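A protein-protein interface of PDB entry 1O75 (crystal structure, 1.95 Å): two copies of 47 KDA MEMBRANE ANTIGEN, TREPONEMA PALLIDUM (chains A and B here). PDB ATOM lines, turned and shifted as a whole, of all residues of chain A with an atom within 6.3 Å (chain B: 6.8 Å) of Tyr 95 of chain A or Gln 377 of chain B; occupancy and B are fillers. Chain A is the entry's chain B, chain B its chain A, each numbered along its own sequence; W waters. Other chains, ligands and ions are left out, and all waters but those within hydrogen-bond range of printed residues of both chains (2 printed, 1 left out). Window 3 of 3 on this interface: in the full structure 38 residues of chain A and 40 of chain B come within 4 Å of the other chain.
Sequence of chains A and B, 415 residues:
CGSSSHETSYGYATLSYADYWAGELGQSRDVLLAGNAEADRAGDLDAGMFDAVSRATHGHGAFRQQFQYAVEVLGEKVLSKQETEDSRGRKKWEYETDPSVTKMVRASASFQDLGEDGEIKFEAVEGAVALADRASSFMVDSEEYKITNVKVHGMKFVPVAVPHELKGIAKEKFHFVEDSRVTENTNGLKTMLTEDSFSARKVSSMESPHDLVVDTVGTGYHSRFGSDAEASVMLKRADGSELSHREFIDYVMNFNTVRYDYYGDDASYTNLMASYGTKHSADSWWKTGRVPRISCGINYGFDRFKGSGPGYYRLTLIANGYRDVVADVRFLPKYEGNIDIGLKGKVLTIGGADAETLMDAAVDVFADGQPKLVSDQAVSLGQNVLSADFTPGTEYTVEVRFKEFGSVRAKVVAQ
The backbone carbonyl oxygen of Ser 375 of chain B lies within hydrogen-bond range of the side-chain amino group of Lys 146 of chain A, at 2.9 Å.
O of Asp 376 of chain B is in hydrogen-bond range of N of Tyr 95 of chain A, 2.9 Å away.
NE2 of Gln 377 of chain B lies within hydrogen-bond range of O of Tyr 95 of chain A.
The backbone NH (N) of Ala 378 of chain B sits at hydrogen-bond distance from the backbone carbonyl oxygen (O) of Tyr 95 of chain A (3.0 Å).
The guanidinium group of Arg 401 of chain B lies within salt-bridge range of the side-chain carboxylate of Glu 94 of chain A (3.2 Å).
The backbone carbonyl oxygen of Ala 361 of chain B lies within hydrogen-bond range of the backbone NH of Val 379 of chain B, at 3.0 Å.
O of Val 363 of chain B lies within hydrogen-bond range of N of Asp 376 of chain B, at 3.5 Å.
The backbone NH (N) of Val 363 of chain B is in hydrogen-bond range of the backbone carbonyl oxygen (O) of Gln 377 of chain B, 2.8 Å away.
The backbone NH (N) of Asp 376 of chain B lies within hydrogen-bond range of the side-chain carboxylate (OD1) of Asp 364 of chain B (2.9 Å).
OD1 of Asp 376 of chain B lies within salt-bridge range of NH2 of Arg 401 of chain B, at 3.5 Å.
OG of Ser 136 of chain A lies within hydrogen-bond range of OH of Tyr 95 of chain A, at 2.7 Å.
Gln 82 of chain A touches Ala 361 of chain B.
Gln 82 of chain A touches Ala 378 of chain B (OE1 to CB, 3.6 Å).
Trp 93 of chain A touches Asp 376 of chain B.
CD of Glu 94 of chain A touches CB of Ala 362 of chain B (3.1 Å).
CA of Glu 94 of chain A touches O of Asp 376 of chain B (3.4 Å).
O of Asp 376 of chain B touches NZ of Lys 146 of chain A (3.8 Å).
Of chain B, only Asp 376, Gln 377 and Ala 378 come within 4 Å of Tyr 95 of chain A.
Glu 96 of chain A touches none of the printed residues of chain B.
Printed residues of chain A within 4 Å of Ala 361 of chain B: Gln 82 (3.6 Å).
Printed residues of chain A within 4 Å of Ser 375 of chain B: Lys 146 (2.9 Å).
Gln 377 of chain B touches just one residue of chain A: Tyr 95.
Val 379 of chain B touches none of the printed residues of chain A.
Printed residues of chain A within 4 Å of Arg 401 of chain B: Glu 94.
The nearest residue of chain B that does not touch Tyr 95 of chain A is Val 379 of chain B (5.8 Å).
Printed residues of chain A that touch a printed residue of chain B: Gln 82, Trp 93, Glu 94, Tyr 95 and Lys 146.
Hydrophobic or aromatic side chains of chain B that line the printed part of chain A: Ala 362 and Ala 378.
Among the printed residues, 11 pairs touch across the chains.
No position is printed for both chains.
Of the 11 pairs that touch across the chains among the printed residues, none has its exchanged pair printed and touching as well.
Water W2 lies within hydrogen-bond range of the side-chain carboxylate (OD2) of Asp 376 of chain B and the backbone carbonyl oxygen (O) of Trp 93 of chain A.
Water W1 bridges the side-chain amide nitrogen of Gln 377 of chain B (2.7 Å) and the backbone NH of Thr 97 of chain A (3.1 Å).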
ATOM      1  N   VAL A  78       4.241  20.120 -24.878  1.00  0.00           N
ATOM      2  CA  VAL A  78       2.785  20.231 -24.749  1.00  0.00           C
ATOM      3  C   VAL A  78       2.130  20.278 -26.141  1.00  0.00           C
ATOM      4  O   VAL A  78       2.539  21.075 -26.982  1.00  0.00           O
ATOM      5  CB  VAL A  78       2.405  21.525 -24.003  1.00  0.00           C
ATOM      6  CG1 VAL A  78       0.915  21.769 -24.118  1.00  0.00           C
ATOM      7  CG2 VAL A  78       2.823  21.414 -22.522  1.00  0.00           C
ATOM      8  N   SER A  80      -1.500  20.053 -26.198  1.00  0.00           N
ATOM      9  CA  SER A  80      -2.751  20.776 -25.954  1.00  0.00           C
ATOM     10  C   SER A  80      -2.953  20.966 -24.474  1.00  0.00           C
ATOM     11  O   SER A  80      -2.392  20.226 -23.666  1.00  0.00           O
ATOM     12  CB  SER A  80      -3.959  20.028 -26.530  1.00  0.00           C
ATOM     13  OG  SER A  80      -4.340  18.947 -25.706  1.00  0.00           O
ATOM     14  N   LYS A  81      -3.718  21.980 -24.109  1.00  0.00           N
ATOM     15  CA  LYS A  81      -3.999  22.179 -22.705  1.00  0.00           C
ATOM     16  C   LYS A  81      -5.318  22.908 -22.534  1.00  0.00           C
ATOM     17  O   LYS A  81      -5.776  23.609 -23.447  1.00  0.00           O
ATOM     18  CB  LYS A  81      -2.846  22.887 -22.000  1.00  0.00           C
ATOM     19  CG  LYS A  81      -2.555  24.308 -22.372  1.00  0.00           C
ATOM     20  CD  LYS A  81      -1.581  24.828 -21.323  1.00  0.00           C
ATOM     21  CE  LYS A  81      -1.264  26.291 -21.464  1.00  0.00           C
ATOM     22  NZ  LYS A  81      -0.301  26.718 -20.402  1.00  0.00           N
ATOM     23  N   GLN A  82      -5.934  22.695 -21.370  1.00  0.00           N
ATOM     24  CA  GLN A  82      -7.234  23.247 -21.044  1.00  0.00           C
ATOM     25  C   GLN A  82      -7.195  23.761 -19.602  1.00  0.00           C
ATOM     26  O   GLN A  82      -6.591  23.132 -18.720  1.00  0.00           O
ATOM     27  CB  GLN A  82      -8.290  22.138 -21.208  1.00  0.00           C
ATOM     28  CG  GLN A  82      -7.857  20.817 -20.520  1.00  0.00           C
ATOM     29  CD  GLN A  82      -8.666  19.570 -20.932  1.00  0.00           C
ATOM     30  OE1 GLN A  82      -8.623  19.125 -22.091  1.00  0.00           O
ATOM     31  NE2 GLN A  82      -9.393  18.997 -19.971  1.00  0.00           N
ATOM     32  N   TRP A  93      -3.966  23.844 -15.070  1.00  0.00           N
ATOM     33  CA  TRP A  93      -4.051  23.323 -16.438  1.00  0.00           C
ATOM     34  C   TRP A  93      -3.929  21.819 -16.557  1.00  0.00           C
ATOM     35  O   TRP A  93      -3.172  21.197 -15.820  1.00  0.00           O
ATOM     36  CB  TRP A  93      -2.973  23.994 -17.293  1.00  0.00           C
ATOM     37  CG  TRP A  93      -3.262  25.439 -17.488  1.00  0.00           C
ATOM     38  CD1 TRP A  93      -3.978  25.994 -18.512  1.00  0.00           C
ATOM     39  CD2 TRP A  93      -3.022  26.496 -16.541  1.00  0.00           C
ATOM     40  NE1 TRP A  93      -4.214  27.329 -18.252  1.00  0.00           N
ATOM     41  CE2 TRP A  93      -3.641  27.661 -17.050  1.00  0.00           C
ATOM     42  CE3 TRP A  93      -2.350  26.569 -15.307  1.00  0.00           C
ATOM     43  CZ2 TRP A  93      -3.612  28.895 -16.364  1.00  0.00           C
ATOM     44  CZ3 TRP A  93      -2.319  27.801 -14.622  1.00  0.00           C
ATOM     45  CH2 TRP A  93      -2.950  28.943 -15.159  1.00  0.00           C
ATOM     46  N   GLU A  94      -4.680  21.244 -17.498  1.00  0.00           N
ATOM     47  CA  GLU A  94      -4.667  19.812 -17.756  1.00  0.00           C
ATOM     48  C   GLU A  94      -4.052  19.743 -19.160  1.00  0.00           C
ATOM     49  O   GLU A  94      -4.405  20.525 -20.037  1.00  0.00           O
ATOM     50  CB  GLU A  94      -6.072  19.253 -17.677  1.00  0.00           C
ATOM     51  CG  GLU A  94      -6.418  18.993 -16.209  1.00  0.00           C
ATOM     52  CD  GLU A  94      -7.883  18.969 -15.944  1.00  0.00           C
ATOM     53  OE1 GLU A  94      -8.261  18.690 -14.781  1.00  0.00           O
ATOM     54  OE2 GLU A  94      -8.649  19.230 -16.896  1.00  0.00           O
ATOM     55  N   TYR A  95      -3.133  18.807 -19.348  1.00  0.00           N
ATOM     56  CA  TYR A  95      -2.359  18.718 -20.573  1.00  0.00           C
ATOM     57  C   TYR A  95      -2.365  17.426 -21.353  1.00  0.00           C
ATOM     58  O   TYR A  95      -2.746  16.366 -20.864  1.00  0.00           O
ATOM     59  CB  TYR A  95      -0.883  18.953 -20.250  1.00  0.00           C
ATOM     60  CG  TYR A  95      -0.517  20.211 -19.519  1.00  0.00           C
ATOM     61  CD1 TYR A  95      -0.062  21.318 -20.216  1.00  0.00           C
ATOM     62  CD2 TYR A  95      -0.535  20.275 -18.116  1.00  0.00           C
ATOM     63  CE1 TYR A  95       0.379  22.458 -19.559  1.00  0.00           C
ATOM     64  CE2 TYR A  95      -0.095  21.429 -17.440  1.00  0.00           C
ATOM     65  CZ  TYR A  95       0.361  22.510 -18.173  1.00  0.00           C
ATOM     66  OH  TYR A  95       0.793  23.671 -17.569  1.00  0.00           O
ATOM     67  N   GLU A  96      -1.862  17.560 -22.581  1.00  0.00           N
ATOM     68  CA  GLU A  96      -1.646  16.451 -23.497  1.00  0.00           C
ATOM     69  C   GLU A  96      -0.214  16.745 -23.940  1.00  0.00           C
ATOM     70  O   GLU A  96       0.127  17.898 -24.262  1.00  0.00           O
ATOM     71  CB  GLU A  96      -2.612  16.510 -24.674  1.00  0.00           C
ATOM     72  CG  GLU A  96      -2.656  15.223 -25.468  1.00  0.00           C
ATOM     73  CD  GLU A  96      -3.623  15.291 -26.640  1.00  0.00           C
ATOM     74  OE1 GLU A  96      -4.776  15.738 -26.431  1.00  0.00           O
ATOM     75  OE2 GLU A  96      -3.225  14.891 -27.762  1.00  0.00           O
ATOM     76  N   THR A  97       0.654  15.740 -23.910  1.00  0.00           N
ATOM     77  CA  THR A  97       2.040  15.987 -24.288  1.00  0.00           C
ATOM     78  C   THR A  97       2.570  14.940 -25.251  1.00  0.00           C
ATOM     79  O   THR A  97       1.949  13.931 -25.477  1.00  0.00           O
ATOM     80  CB  THR A  97       2.965  15.942 -23.070  1.00  0.00           C
ATOM     81  OG1 THR A  97       3.089  14.576 -22.641  1.00  0.00           O
ATOM     82  CG2 THR A  97       2.390  16.782 -21.925  1.00  0.00           C
ATOM     83  N   ALA A 135       3.745  26.221 -10.756  1.00  0.00           N
ATOM     84  CA  ALA A 135       4.022  25.899 -12.161  1.00  0.00           C
ATOM     85  C   ALA A 135       3.947  24.421 -12.478  1.00  0.00           C
ATOM     86  O   ALA A 135       4.374  23.585 -11.697  1.00  0.00           O
ATOM     87  CB  ALA A 135       5.406  26.422 -12.552  1.00  0.00           C
ATOM     88  N   SER A 136       3.400  24.097 -13.642  1.00  0.00           N
ATOM     89  CA  SER A 136       3.327  22.717 -14.068  1.00  0.00           C
ATOM     90  C   SER A 136       4.047  22.584 -15.419  1.00  0.00           C
ATOM     91  O   SER A 136       4.164  21.499 -15.966  1.00  0.00           O
ATOM     92  CB  SER A 136       1.865  22.286 -14.176  1.00  0.00           C
ATOM     93  OG  SER A 136       1.153  23.256 -14.924  1.00  0.00           O
ATOM     94  N   SER A 137       4.541  23.697 -15.939  1.00  0.00           N
ATOM     95  CA  SER A 137       5.246  23.677 -17.223  1.00  0.00           C
ATOM     96  C   SER A 137       6.223  24.835 -17.282  1.00  0.00           C
ATOM     97  O   SER A 137       6.232  25.689 -16.398  1.00  0.00           O
ATOM     98  CB  SER A 137       4.236  23.815 -18.373  1.00  0.00           C
ATOM     99  OG  SER A 137       3.688  25.128 -18.373  1.00  0.00           O
ATOM    100  N   GLU A 144       6.203  25.326 -25.038  1.00  0.00           N
ATOM    101  CA  GLU A 144       5.907  24.935 -23.664  1.00  0.00           C
ATOM    102  C   GLU A 144       6.094  23.441 -23.416  1.00  0.00           C
ATOM    103  O   GLU A 144       5.777  22.603 -24.264  1.00  0.00           O
ATOM    104  CB  GLU A 144       4.469  25.355 -23.315  1.00  0.00           C
ATOM    105  CG  GLU A 144       4.063  25.157 -21.855  1.00  0.00           C
ATOM    106  CD  GLU A 144       2.609  25.527 -21.599  1.00  0.00           C
ATOM    107  OE1 GLU A 144       1.881  25.774 -22.581  1.00  0.00           O
ATOM    108  OE2 GLU A 144       2.190  25.561 -20.424  1.00  0.00           O
ATOM    109  N   TYR A 145       6.608  23.118 -22.232  1.00  0.00           N
ATOM    110  CA  TYR A 145       6.851  21.733 -21.845  1.00  0.00           C
ATOM    111  C   TYR A 145       6.276  21.486 -20.461  1.00  0.00           C
ATOM    112  O   TYR A 145       6.466  22.298 -19.580  1.00  0.00           O
ATOM    113  CB  TYR A 145       8.357  21.467 -21.818  1.00  0.00           C
ATOM    114  CG  TYR A 145       9.015  21.555 -23.175  1.00  0.00           C
ATOM    115  CD1 TYR A 145       9.101  20.435 -24.000  1.00  0.00           C
ATOM    116  CD2 TYR A 145       9.529  22.764 -23.643  1.00  0.00           C
ATOM    117  CE1 TYR A 145       9.680  20.514 -25.257  1.00  0.00           C
ATOM    118  CE2 TYR A 145      10.110  22.854 -24.903  1.00  0.00           C
ATOM    119  CZ  TYR A 145      10.178  21.721 -25.700  1.00  0.00           C
ATOM    120  OH  TYR A 145      10.748  21.811 -26.948  1.00  0.00           O
ATOM    121  N   LYS A 146       5.576  20.372 -20.293  1.00  0.00           N
ATOM    122  CA  LYS A 146       4.992  20.003 -19.010  1.00  0.00           C
ATOM    123  C   LYS A 146       6.071  19.324 -18.152  1.00  0.00           C
ATOM    124  O   LYS A 146       6.638  18.301 -18.548  1.00  0.00           O
ATOM    125  CB  LYS A 146       3.842  19.028 -19.222  1.00  0.00           C
ATOM    126  CG  LYS A 146       3.213  18.469 -17.938  1.00  0.00           C
ATOM    127  CD  LYS A 146       2.090  17.513 -18.289  1.00  0.00           C
ATOM    128  CE  LYS A 146       1.946  16.355 -17.311  1.00  0.00           C
ATOM    129  NZ  LYS A 146       0.846  16.560 -16.325  1.00  0.00           N
ATOM    130  N   LEU B 348      -4.315   4.137 -21.458  1.00  0.00           N
ATOM    131  CA  LEU B 348      -5.466   4.218 -20.569  1.00  0.00           C
ATOM    132  C   LEU B 348      -6.696   4.260 -21.484  1.00  0.00           C
ATOM    133  O   LEU B 348      -6.827   5.146 -22.332  1.00  0.00           O
ATOM    134  CB  LEU B 348      -5.403   5.474 -19.688  1.00  0.00           C
ATOM    135  CG  LEU B 348      -6.446   5.543 -18.553  1.00  0.00           C
ATOM    136  CD1 LEU B 348      -6.035   6.588 -17.534  1.00  0.00           C
ATOM    137  CD2 LEU B 348      -7.816   5.856 -19.107  1.00  0.00           C
ATOM    138  N   ALA B 361     -12.343  16.015 -20.555  1.00  0.00           N
ATOM    139  CA  ALA B 361     -12.216  15.223 -19.333  1.00  0.00           C
ATOM    140  C   ALA B 361     -10.732  15.144 -18.979  1.00  0.00           C
ATOM    141  O   ALA B 361      -9.874  15.411 -19.821  1.00  0.00           O
ATOM    142  CB  ALA B 361     -12.771  13.823 -19.541  1.00  0.00           C
ATOM    143  N   ALA B 362     -10.429  14.806 -17.731  1.00  0.00           N
ATOM    144  CA  ALA B 362      -9.039  14.683 -17.324  1.00  0.00           C
ATOM    145  C   ALA B 362      -8.956  13.623 -16.236  1.00  0.00           C
ATOM    146  O   ALA B 362      -9.967  13.283 -15.624  1.00  0.00           O
ATOM    147  CB  ALA B 362      -8.522  16.013 -16.799  1.00  0.00           C
ATOM    148  N   VAL B 363      -7.754  13.099 -16.003  1.00  0.00           N
ATOM    149  CA  VAL B 363      -7.584  12.076 -14.982  1.00  0.00           C
ATOM    150  C   VAL B 363      -6.314  12.230 -14.168  1.00  0.00           C
ATOM    151  O   VAL B 363      -5.381  12.955 -14.535  1.00  0.00           O
ATOM    152  CB  VAL B 363      -7.539  10.631 -15.589  1.00  0.00           C
ATOM    153  CG1 VAL B 363      -8.845  10.286 -16.287  1.00  0.00           C
ATOM    154  CG2 VAL B 363      -6.370  10.516 -16.551  1.00  0.00           C
ATOM    155  N   ASP B 364      -6.312  11.535 -13.037  1.00  0.00           N
ATOM    156  CA  ASP B 364      -5.161  11.459 -12.143  1.00  0.00           C
ATOM    157  C   ASP B 364      -5.097   9.950 -11.912  1.00  0.00           C
ATOM    158  O   ASP B 364      -6.135   9.292 -11.866  1.00  0.00           O
ATOM    159  CB  ASP B 364      -5.417  12.132 -10.788  1.00  0.00           C
ATOM    160  CG  ASP B 364      -5.326  13.655 -10.835  1.00  0.00           C
ATOM    161  OD1 ASP B 364      -4.634  14.220 -11.714  1.00  0.00           O
ATOM    162  OD2 ASP B 364      -5.940  14.287  -9.947  1.00  0.00           O
ATOM    163  N   VAL B 365      -3.899   9.390 -11.791  1.00  0.00           N
ATOM    164  CA  VAL B 365      -3.790   7.957 -11.514  1.00  0.00           C
ATOM    165  C   VAL B 365      -2.714   7.798 -10.459  1.00  0.00           C
ATOM    166  O   VAL B 365      -1.628   8.363 -10.587  1.00  0.00           O
ATOM    167  CB  VAL B 365      -3.372   7.125 -12.751  1.00  0.00           C
ATOM    168  CG1 VAL B 365      -3.467   5.642 -12.417  1.00  0.00           C
ATOM    169  CG2 VAL B 365      -4.259   7.456 -13.949  1.00  0.00           C
ATOM    170  N   VAL B 374       0.113   9.673 -12.681  1.00  0.00           N
ATOM    171  CA  VAL B 374      -0.466  10.484 -13.755  1.00  0.00           C
ATOM    172  C   VAL B 374      -1.244  11.634 -13.122  1.00  0.00           C
ATOM    173  O   VAL B 374      -2.040  11.402 -12.229  1.00  0.00           O
ATOM    174  CB  VAL B 374      -1.450   9.641 -14.598  1.00  0.00           C
ATOM    175  CG1 VAL B 374      -2.255  10.543 -15.528  1.00  0.00           C
ATOM    176  CG2 VAL B 374      -0.688   8.588 -15.394  1.00  0.00           C
ATOM    177  N   SER B 375      -1.009  12.867 -13.549  1.00  0.00           N
ATOM    178  CA  SER B 375      -1.768  13.988 -12.987  1.00  0.00           C
ATOM    179  C   SER B 375      -2.111  15.040 -14.036  1.00  0.00           C
ATOM    180  O   SER B 375      -1.322  15.288 -14.951  1.00  0.00           O
ATOM    181  CB  SER B 375      -0.990  14.656 -11.852  1.00  0.00           C
ATOM    182  OG  SER B 375       0.302  15.036 -12.287  1.00  0.00           O
ATOM    183  N   ASP B 376      -3.278  15.666 -13.888  1.00  0.00           N
ATOM    184  CA  ASP B 376      -3.723  16.700 -14.828  1.00  0.00           C
ATOM    185  C   ASP B 376      -3.493  16.244 -16.266  1.00  0.00           C
ATOM    186  O   ASP B 376      -2.886  16.949 -17.083  1.00  0.00           O
ATOM    187  CB  ASP B 376      -2.968  17.990 -14.548  1.00  0.00           C
ATOM    188  CG  ASP B 376      -3.082  18.409 -13.100  1.00  0.00           C
ATOM    189  OD1 ASP B 376      -4.117  18.073 -12.490  1.00  0.00           O
ATOM    190  OD2 ASP B 376      -2.151  19.070 -12.589  1.00  0.00           O
ATOM    191  N   GLN B 377      -3.975  15.037 -16.538  1.00  0.00           N
ATOM    192  CA  GLN B 377      -3.850  14.393 -17.831  1.00  0.00           C
ATOM    193  C   GLN B 377      -5.184  14.476 -18.563  1.00  0.00           C
ATOM    194  O   GLN B 377      -6.164  13.843 -18.161  1.00  0.00           O
ATOM    195  CB  GLN B 377      -3.476  12.914 -17.643  1.00  0.00           C
ATOM    196  CG  GLN B 377      -3.337  12.126 -18.934  1.00  0.00           C
ATOM    197  CD  GLN B 377      -2.264  12.697 -19.844  1.00  0.00           C
ATOM    198  OE1 GLN B 377      -1.111  12.877 -19.437  1.00  0.00           O
ATOM    199  NE2 GLN B 377      -2.638  12.987 -21.085  1.00  0.00           N
ATOM    200  N   ALA B 378      -5.214  15.256 -19.640  1.00  0.00           N
ATOM    201  CA  ALA B 378      -6.431  15.398 -20.436  1.00  0.00           C
ATOM    202  C   ALA B 378      -6.645  14.068 -21.146  1.00  0.00           C
ATOM    203  O   ALA B 378      -5.686  13.424 -21.563  1.00  0.00           O
ATOM    204  CB  ALA B 378      -6.253  16.540 -21.475  1.00  0.00           C
ATOM    205  N   VAL B 379      -7.893  13.643 -21.271  1.00  0.00           N
ATOM    206  CA  VAL B 379      -8.188  12.386 -21.947  1.00  0.00           C
ATOM    207  C   VAL B 379      -9.521  12.508 -22.702  1.00  0.00           C
ATOM    208  O   VAL B 379     -10.227  13.511 -22.573  1.00  0.00           O
ATOM    209  CB  VAL B 379      -8.304  11.205 -20.940  1.00  0.00           C
ATOM    210  CG1 VAL B 379      -7.041  11.108 -20.091  1.00  0.00           C
ATOM    211  CG2 VAL B 379      -9.524  11.378 -20.065  1.00  0.00           C
ATOM    212  N   ASN B 384      -6.014   6.139 -24.680  1.00  0.00           N
ATOM    213  CA  ASN B 384      -5.204   7.313 -24.386  1.00  0.00           C
ATOM    214  C   ASN B 384      -3.767   6.839 -24.111  1.00  0.00           C
ATOM    215  O   ASN B 384      -3.488   6.231 -23.067  1.00  0.00           O
ATOM    216  CB  ASN B 384      -5.772   8.045 -23.160  1.00  0.00           C
ATOM    217  CG  ASN B 384      -7.156   8.635 -23.412  1.00  0.00           C
ATOM    218  OD1 ASN B 384      -7.283   9.717 -23.987  1.00  0.00           O
ATOM    219  ND2 ASN B 384      -8.199   7.924 -22.982  1.00  0.00           N
ATOM    220  N   VAL B 385      -2.874   7.106 -25.064  1.00  0.00           N
ATOM    221  CA  VAL B 385      -1.467   6.722 -24.961  1.00  0.00           C
ATOM    222  C   VAL B 385      -0.759   7.700 -24.036  1.00  0.00           C
ATOM    223  O   VAL B 385      -0.532   8.856 -24.404  1.00  0.00           O
ATOM    224  CB  VAL B 385      -0.774   6.769 -26.344  1.00  0.00           C
ATOM    225  CG1 VAL B 385       0.653   6.267 -26.234  1.00  0.00           C
ATOM    226  CG2 VAL B 385      -1.561   5.937 -27.341  1.00  0.00           C
ATOM    227  N   LEU B 386      -0.399   7.236 -22.843  1.00  0.00           N
ATOM    228  CA  LEU B 386       0.255   8.100 -21.875  1.00  0.00           C
ATOM    229  C   LEU B 386       1.776   8.007 -21.849  1.00  0.00           C
ATOM    230  O   LEU B 386       2.391   7.290 -22.643  1.00  0.00           O
ATOM    231  CB  LEU B 386      -0.317   7.833 -20.488  1.00  0.00           C
ATOM    232  CG  LEU B 386      -1.835   8.027 -20.445  1.00  0.00           C
ATOM    233  CD1 LEU B 386      -2.343   7.812 -19.034  1.00  0.00           C
ATOM    234  CD2 LEU B 386      -2.189   9.421 -20.937  1.00  0.00           C
ATOM    235  N   SER B 387       2.380   8.748 -20.932  1.00  0.00           N
ATOM    236  CA  SER B 387       3.826   8.773 -20.819  1.00  0.00           C
ATOM    237  C   SER B 387       4.338   7.738 -19.826  1.00  0.00           C
ATOM    238  O   SER B 387       5.415   7.164 -20.008  1.00  0.00           O
ATOM    239  CB  SER B 387       4.275  10.171 -20.401  1.00  0.00           C
ATOM    240  OG  SER B 387       5.670  10.216 -20.180  1.00  0.00           O
ATOM    241  N   ARG B 401     -12.192  13.343 -13.921  1.00  0.00           N
ATOM    242  CA  ARG B 401     -12.873  14.610 -13.682  1.00  0.00           C
ATOM    243  C   ARG B 401     -13.620  15.013 -14.960  1.00  0.00           C
ATOM    244  O   ARG B 401     -13.022  15.139 -16.030  1.00  0.00           O
ATOM    245  CB  ARG B 401     -11.872  15.710 -13.294  1.00  0.00           C
ATOM    246  CG  ARG B 401     -11.207  15.498 -11.928  1.00  0.00           C
ATOM    247  CD  ARG B 401     -10.318  16.679 -11.544  1.00  0.00           C
ATOM    248  NE  ARG B 401      -9.118  16.787 -12.376  1.00  0.00           N
ATOM    249  CZ  ARG B 401      -8.069  15.966 -12.302  1.00  0.00           C
ATOM    250  NH1 ARG B 401      -8.061  14.966 -11.428  1.00  0.00           N
ATOM    251  NH2 ARG B 401      -7.022  16.148 -13.097  1.00  0.00           N
HETATM  252  O   HOH W   1      -0.860  13.147 -23.157  1.00  0.00           O
HETATM  253  O   HOH W   2      -1.554  21.422 -13.650  1.00  0.00           O
